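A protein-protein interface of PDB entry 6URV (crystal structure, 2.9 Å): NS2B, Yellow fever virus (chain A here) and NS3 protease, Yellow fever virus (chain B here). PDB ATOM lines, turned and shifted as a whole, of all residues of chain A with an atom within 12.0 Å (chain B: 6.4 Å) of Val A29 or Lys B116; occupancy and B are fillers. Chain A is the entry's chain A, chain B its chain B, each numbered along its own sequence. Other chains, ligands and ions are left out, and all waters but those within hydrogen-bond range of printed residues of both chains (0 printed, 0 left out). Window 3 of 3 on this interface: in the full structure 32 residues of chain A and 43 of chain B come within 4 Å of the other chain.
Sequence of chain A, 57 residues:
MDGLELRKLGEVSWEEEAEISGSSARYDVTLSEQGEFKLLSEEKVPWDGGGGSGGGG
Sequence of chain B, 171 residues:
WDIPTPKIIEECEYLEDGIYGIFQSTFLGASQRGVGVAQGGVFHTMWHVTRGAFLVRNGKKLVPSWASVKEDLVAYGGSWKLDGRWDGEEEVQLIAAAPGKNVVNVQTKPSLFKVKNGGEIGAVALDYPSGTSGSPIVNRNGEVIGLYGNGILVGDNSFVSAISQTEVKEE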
ATOM      1  N   ALA A  25       2.962 -21.104 -25.493  1.00  0.00           N
ATOM      2  CA  ALA A  25       3.607 -20.515 -26.658  1.00  0.00           C
ATOM      3  C   ALA A  25       5.101 -20.417 -26.389  1.00  0.00           C
ATOM      4  O   ALA A  25       5.549 -20.509 -25.245  1.00  0.00           O
ATOM      5  CB  ALA A  25       3.023 -19.137 -26.987  1.00  0.00           C
ATOM      6  N   ARG A  26       5.871 -20.239 -27.458  1.00  0.00           N
ATOM      7  CA  ARG A  26       7.316 -20.099 -27.358  1.00  0.00           C
ATOM      8  C   ARG A  26       7.730 -18.687 -27.750  1.00  0.00           C
ATOM      9  O   ARG A  26       7.334 -18.193 -28.810  1.00  0.00           O
ATOM     10  CB  ARG A  26       8.029 -21.123 -28.244  1.00  0.00           C
ATOM     11  CG  ARG A  26       7.823 -22.569 -27.813  1.00  0.00           C
ATOM     12  CD  ARG A  26       8.543 -23.536 -28.743  1.00  0.00           C
ATOM     13  NE  ARG A  26       9.764 -22.961 -29.303  1.00  0.00           N
ATOM     14  CZ  ARG A  26      10.945 -23.573 -29.314  1.00  0.00           C
ATOM     15  NH1 ARG A  26      12.000 -22.970 -29.845  1.00  0.00           N
ATOM     16  NH2 ARG A  26      11.072 -24.786 -28.794  1.00  0.00           N
ATOM     17  N   TYR A  27       8.519 -18.043 -26.890  1.00  0.00           N
ATOM     18  CA  TYR A  27       9.010 -16.690 -27.122  1.00  0.00           C
ATOM     19  C   TYR A  27      10.520 -16.709 -26.961  1.00  0.00           C
ATOM     20  O   TYR A  27      11.030 -17.318 -26.016  1.00  0.00           O
ATOM     21  CB  TYR A  27       8.417 -15.672 -26.134  1.00  0.00           C
ATOM     22  CG  TYR A  27       6.912 -15.691 -25.948  1.00  0.00           C
ATOM     23  CD1 TYR A  27       6.279 -16.727 -25.273  1.00  0.00           C
ATOM     24  CD2 TYR A  27       6.129 -14.641 -26.410  1.00  0.00           C
ATOM     25  CE1 TYR A  27       4.906 -16.732 -25.094  1.00  0.00           C
ATOM     26  CE2 TYR A  27       4.758 -14.643 -26.240  1.00  0.00           C
ATOM     27  CZ  TYR A  27       4.151 -15.683 -25.575  1.00  0.00           C
ATOM     28  OH  TYR A  27       2.786 -15.675 -25.401  1.00  0.00           O
ATOM     29  N   ASP A  28      11.242 -16.053 -27.866  1.00  0.00           N
ATOM     30  CA  ASP A  28      12.678 -15.885 -27.695  1.00  0.00           C
ATOM     31  C   ASP A  28      12.964 -14.462 -27.230  1.00  0.00           C
ATOM     32  O   ASP A  28      12.565 -13.492 -27.882  1.00  0.00           O
ATOM     33  CB  ASP A  28      13.478 -16.235 -28.954  1.00  0.00           C
ATOM     34  CG  ASP A  28      12.807 -15.798 -30.228  1.00  0.00           C
ATOM     35  OD1 ASP A  28      11.949 -14.895 -30.183  1.00  0.00           O
ATOM     36  OD2 ASP A  28      13.154 -16.365 -31.289  1.00  0.00           O
ATOM     37  N   VAL A  29      13.656 -14.351 -26.098  1.00  0.00           N
ATOM     38  CA  VAL A  29      13.815 -13.104 -25.368  1.00  0.00           C
ATOM     39  C   VAL A  29      15.289 -12.908 -25.047  1.00  0.00           C
ATOM     40  O   VAL A  29      16.090 -13.842 -25.099  1.00  0.00           O
ATOM     41  CB  VAL A  29      12.975 -13.070 -24.074  1.00  0.00           C
ATOM     42  CG1 VAL A  29      11.509 -12.879 -24.409  1.00  0.00           C
ATOM     43  CG2 VAL A  29      13.190 -14.335 -23.262  1.00  0.00           C
ATOM     44  N   THR A  30      15.642 -11.672 -24.711  1.00  0.00           N
ATOM     45  CA  THR A  30      16.973 -11.371 -24.213  1.00  0.00           C
ATOM     46  C   THR A  30      16.896 -11.143 -22.710  1.00  0.00           C
ATOM     47  O   THR A  30      15.899 -10.635 -22.188  1.00  0.00           O
ATOM     48  CB  THR A  30      17.559 -10.133 -24.898  1.00  0.00           C
ATOM     49  OG1 THR A  30      18.754  -9.727 -24.219  1.00  0.00           O
ATOM     50  CG2 THR A  30      16.561  -8.980 -24.876  1.00  0.00           C
ATOM     51  N   LEU A  31      17.957 -11.539 -22.015  1.00  0.00           N
ATOM     52  CA  LEU A  31      18.054 -11.375 -20.572  1.00  0.00           C
ATOM     53  C   LEU A  31      19.284 -10.552 -20.229  1.00  0.00           C
ATOM     54  O   LEU A  31      20.405 -10.928 -20.587  1.00  0.00           O
ATOM     55  CB  LEU A  31      18.112 -12.729 -19.867  1.00  0.00           C
ATOM     56  CG  LEU A  31      18.401 -12.632 -18.370  1.00  0.00           C
ATOM     57  CD1 LEU A  31      17.181 -12.100 -17.637  1.00  0.00           C
ATOM     58  CD2 LEU A  31      18.822 -13.978 -17.812  1.00  0.00           C
ATOM     59  N   SER A  32      19.070  -9.435 -19.545  1.00  0.00           N
ATOM     60  CA  SER A  32      20.159  -8.588 -19.097  1.00  0.00           C
ATOM     61  C   SER A  32      20.794  -9.165 -17.833  1.00  0.00           C
ATOM     62  O   SER A  32      20.264 -10.078 -17.192  1.00  0.00           O
ATOM     63  CB  SER A  32      19.665  -7.166 -18.844  1.00  0.00           C
ATOM     64  OG  SER A  32      18.892  -7.096 -17.658  1.00  0.00           O
ATOM     65  N   GLU A  33      21.955  -8.617 -17.476  1.00  0.00           N
ATOM     66  CA  GLU A  33      22.608  -9.017 -16.236  1.00  0.00           C
ATOM     67  C   GLU A  33      21.828  -8.575 -15.003  1.00  0.00           C
ATOM     68  O   GLU A  33      22.077  -9.094 -13.910  1.00  0.00           O
ATOM     69  CB  GLU A  33      24.033  -8.466 -16.186  1.00  0.00           C
ATOM     70  CG  GLU A  33      24.880  -8.831 -17.399  1.00  0.00           C
ATOM     71  CD  GLU A  33      25.395 -10.263 -17.368  1.00  0.00           C
ATOM     72  OE1 GLU A  33      24.824 -11.105 -16.640  1.00  0.00           O
ATOM     73  OE2 GLU A  33      26.379 -10.551 -18.081  1.00  0.00           O
ATOM     74  N   GLY A  35      18.666  -9.161 -14.620  1.00  0.00           N
ATOM     75  CA  GLY A  35      17.502 -10.013 -14.499  1.00  0.00           C
ATOM     76  C   GLY A  35      16.292  -9.527 -15.259  1.00  0.00           C
ATOM     77  O   GLY A  35      15.180  -9.999 -15.001  1.00  0.00           O
ATOM     78  N   GLU A  36      16.478  -8.600 -16.194  1.00  0.00           N
ATOM     79  CA  GLU A  36      15.387  -8.054 -16.989  1.00  0.00           C
ATOM     80  C   GLU A  36      15.159  -8.911 -18.226  1.00  0.00           C
ATOM     81  O   GLU A  36      16.110  -9.355 -18.876  1.00  0.00           O
ATOM     82  CB  GLU A  36      15.698  -6.609 -17.390  1.00  0.00           C
ATOM     83  CG  GLU A  36      14.569  -5.862 -18.087  1.00  0.00           C
ATOM     84  CD  GLU A  36      14.983  -4.461 -18.518  1.00  0.00           C
ATOM     85  OE1 GLU A  36      16.023  -3.971 -18.024  1.00  0.00           O
ATOM     86  OE2 GLU A  36      14.274  -3.853 -19.350  1.00  0.00           O
ATOM     87  N   PHE A  37      13.890  -9.110 -18.565  1.00  0.00           N
ATOM     88  CA  PHE A  37      13.493  -9.890 -19.726  1.00  0.00           C
ATOM     89  C   PHE A  37      12.857  -8.972 -20.762  1.00  0.00           C
ATOM     90  O   PHE A  37      12.028  -8.121 -20.422  1.00  0.00           O
ATOM     91  CB  PHE A  37      12.488 -10.977 -19.326  1.00  0.00           C
ATOM     92  CG  PHE A  37      13.113 -12.269 -18.872  1.00  0.00           C
ATOM     93  CD1 PHE A  37      14.116 -12.874 -19.612  1.00  0.00           C
ATOM     94  CD2 PHE A  37      12.672 -12.894 -17.714  1.00  0.00           C
ATOM     95  CE1 PHE A  37      14.680 -14.070 -19.196  1.00  0.00           C
ATOM     96  CE2 PHE A  37      13.232 -14.090 -17.294  1.00  0.00           C
ATOM     97  CZ  PHE A  37      14.236 -14.677 -18.036  1.00  0.00           C
ATOM     98  N   LYS A  38      13.252  -9.136 -22.022  1.00  0.00           N
ATOM     99  CA  LYS A  38      12.677  -8.345 -23.101  1.00  0.00           C
ATOM    100  C   LYS A  38      12.628  -9.193 -24.363  1.00  0.00           C
ATOM    101  O   LYS A  38      13.451 -10.092 -24.548  1.00  0.00           O
ATOM    102  CB  LYS A  38      13.479  -7.061 -23.347  1.00  0.00           C
ATOM    103  N   LEU A  39      11.694  -8.866 -25.251  1.00  0.00           N
ATOM    104  CA  LEU A  39      11.522  -9.616 -26.495  1.00  0.00           C
ATOM    105  C   LEU A  39      12.388  -9.058 -27.618  1.00  0.00           C
ATOM    106  O   LEU A  39      12.728  -9.768 -28.567  1.00  0.00           O
ATOM    107  CB  LEU A  39      10.052  -9.616 -26.923  1.00  0.00           C
ATOM    108  CG  LEU A  39       9.184 -10.791 -26.463  1.00  0.00           C
ATOM    109  CD1 LEU A  39       7.711 -10.402 -26.416  1.00  0.00           C
ATOM    110  CD2 LEU A  39       9.392 -12.000 -27.366  1.00  0.00           C
ATOM    111  N   PHE B 113      10.765 -19.670 -22.794  1.00  0.00           N
ATOM    112  CA  PHE B 113      11.563 -18.491 -23.106  1.00  0.00           C
ATOM    113  C   PHE B 113      12.887 -18.984 -23.678  1.00  0.00           C
ATOM    114  O   PHE B 113      13.669 -19.630 -22.974  1.00  0.00           O
ATOM    115  CB  PHE B 113      11.800 -17.628 -21.868  1.00  0.00           C
ATOM    116  CG  PHE B 113      10.647 -16.730 -21.506  1.00  0.00           C
ATOM    117  CD1 PHE B 113       9.415 -16.862 -22.118  1.00  0.00           C
ATOM    118  CD2 PHE B 113      10.805 -15.755 -20.534  1.00  0.00           C
ATOM    119  CE1 PHE B 113       8.360 -16.031 -21.770  1.00  0.00           C
ATOM    120  CE2 PHE B 113       9.757 -14.925 -20.183  1.00  0.00           C
ATOM    121  CZ  PHE B 113       8.533 -15.065 -20.798  1.00  0.00           C
ATOM    122  N   LYS B 114      13.140 -18.691 -24.948  1.00  0.00           N
ATOM    123  CA  LYS B 114      14.426 -19.000 -25.561  1.00  0.00           C
ATOM    124  C   LYS B 114      15.323 -17.768 -25.471  1.00  0.00           C
ATOM    125  O   LYS B 114      15.118 -16.798 -26.202  1.00  0.00           O
ATOM    126  CB  LYS B 114      14.226 -19.429 -27.014  1.00  0.00           C
ATOM    127  N   VAL B 115      16.333 -17.798 -24.597  1.00  0.00           N
ATOM    128  CA  VAL B 115      17.195 -16.631 -24.415  1.00  0.00           C
ATOM    129  C   VAL B 115      18.313 -16.648 -25.449  1.00  0.00           C
ATOM    130  O   VAL B 115      18.974 -17.674 -25.649  1.00  0.00           O
ATOM    131  CB  VAL B 115      17.769 -16.537 -22.989  1.00  0.00           C
ATOM    132  CG1 VAL B 115      18.367 -17.843 -22.519  1.00  0.00           C
ATOM    133  CG2 VAL B 115      18.834 -15.424 -22.947  1.00  0.00           C
ATOM    134  N   LYS B 116      18.522 -15.507 -26.108  1.00  0.00           N
ATOM    135  CA  LYS B 116      19.616 -15.375 -27.062  1.00  0.00           C
ATOM    136  C   LYS B 116      20.944 -15.682 -26.379  1.00  0.00           C
ATOM    137  O   LYS B 116      21.215 -15.210 -25.269  1.00  0.00           O
ATOM    138  CB  LYS B 116      19.642 -13.969 -27.658  1.00  0.00           C
ATOM    139  N   ASN B 117      21.773 -16.476 -27.057  1.00  0.00           N
ATOM    140  CA  ASN B 117      23.105 -16.847 -26.571  1.00  0.00           C
ATOM    141  C   ASN B 117      23.012 -17.528 -25.207  1.00  0.00           C
ATOM    142  O   ASN B 117      23.796 -17.249 -24.297  1.00  0.00           O
ATOM    143  CB  ASN B 117      24.035 -15.627 -26.507  1.00  0.00           C
ATOM    144  CG  ASN B 117      24.490 -15.154 -27.880  1.00  0.00           C
ATOM    145  OD1 ASN B 117      24.383 -15.876 -28.870  1.00  0.00           O
ATOM    146  ND2 ASN B 117      25.008 -13.931 -27.938  1.00  0.00           N
ATOM    147  N   GLY B 118      22.047 -18.445 -25.070  1.00  0.00           N
ATOM    148  CA  GLY B 118      21.852 -19.184 -23.833  1.00  0.00           C
ATOM    149  C   GLY B 118      21.068 -20.478 -23.974  1.00  0.00           C
ATOM    150  O   GLY B 118      21.258 -21.219 -24.942  1.00  0.00           O
ATOM    151  N   GLY B 119      20.166 -20.750 -23.027  1.00  0.00           N
ATOM    152  CA  GLY B 119      19.383 -21.965 -23.017  1.00  0.00           C
ATOM    153  C   GLY B 119      17.889 -21.711 -22.875  1.00  0.00           C
ATOM    154  O   GLY B 119      17.423 -20.576 -22.885  1.00  0.00           O
ATOM    155  N   ILE B 152       7.819 -10.970 -19.093  1.00  0.00           N
ATOM    156  CA  ILE B 152       7.684  -9.985 -20.155  1.00  0.00           C
ATOM    157  C   ILE B 152       6.213  -9.651 -20.348  1.00  0.00           C
ATOM    158  O   ILE B 152       5.317 -10.363 -19.890  1.00  0.00           O
ATOM    159  CB  ILE B 152       8.263 -10.476 -21.500  1.00  0.00           C
ATOM    160  CG1 ILE B 152       7.562 -11.771 -21.930  1.00  0.00           C
ATOM    161  CG2 ILE B 152       9.763 -10.653 -21.417  1.00  0.00           C
ATOM    162  CD1 ILE B 152       8.221 -12.478 -23.086  1.00  0.00           C
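The backbone NH (N) of Thr A30 sits at hydrogen-bond distance from the backbone carbonyl oxygen (O) of Lys A38 (2.7 Å).
Among the printed residues, pairs that only touch across the chains: Tyr A27 with Phe B113 (3.2 Å), Asp A28 with Lys B114 (3.0 Å), Val A29 with Phe B113 (3.8 Å), Val A29 with Val B115 (3.1 Å), Val A29 with Ile B152 (3.6 Å), Phe A37 with Ile B152 (3.5 Å), Lys A38 with Ile B152 (3.9 Å) and Leu A39 with Ile B152 (3.9 Å).
Hydrophobic or aromatic side chains of chain A within 4 Å of the printed part of chain B: Val A29, Phe A37 and Leu A39. Among the printed residues, 11 pairs touch across the chains.
Of the printed residues of chain B, Tyr A27 touches Phe B113 (3.2 Å) and Lys B114 (2.7 Å). Of the printed residues of chain B, Asp A28 touches Lys B114. Val A29 touches just these residues of chain B: Phe B113 (3.8 Å), Lys B114 (2.9 Å), Val B115 (3.1 Å), Lys B116 (3.1 Å) and Ile B152 (3.6 Å). Phe B113 touches just these residues of chain A: Tyr A27 (3.2 Å) and Val A29 (3.8 Å). Of chain A, only Tyr A27 (2.7 Å), Asp A28 (3.0 Å) and Val A29 (2.9 Å) come within 4 Å of Lys B114. Of chain A, only Val A29 (3.1 Å) comes within 4 Å of Val B115. Of the printed residues of chain A, Lys B116 touches Val A29. No residue of chain A comes within 4 Å of Gly B118. No residue of chain A comes within 4 Å of Gly B119.
The backbone carbonyl oxygen (O) of Tyr A27 lies within hydrogen-bond range of the backbone NH (N) of Lys B114 (2.7 Å). The backbone NH (N) of Val A29 lies within hydrogen-bond range of the backbone carbonyl oxygen (O) of Lys B114, 2.9 Å away. The backbone NH of Lys B116 is in hydrogen-bond range of the backbone carbonyl oxygen of Val A29, at 3.1 Å.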
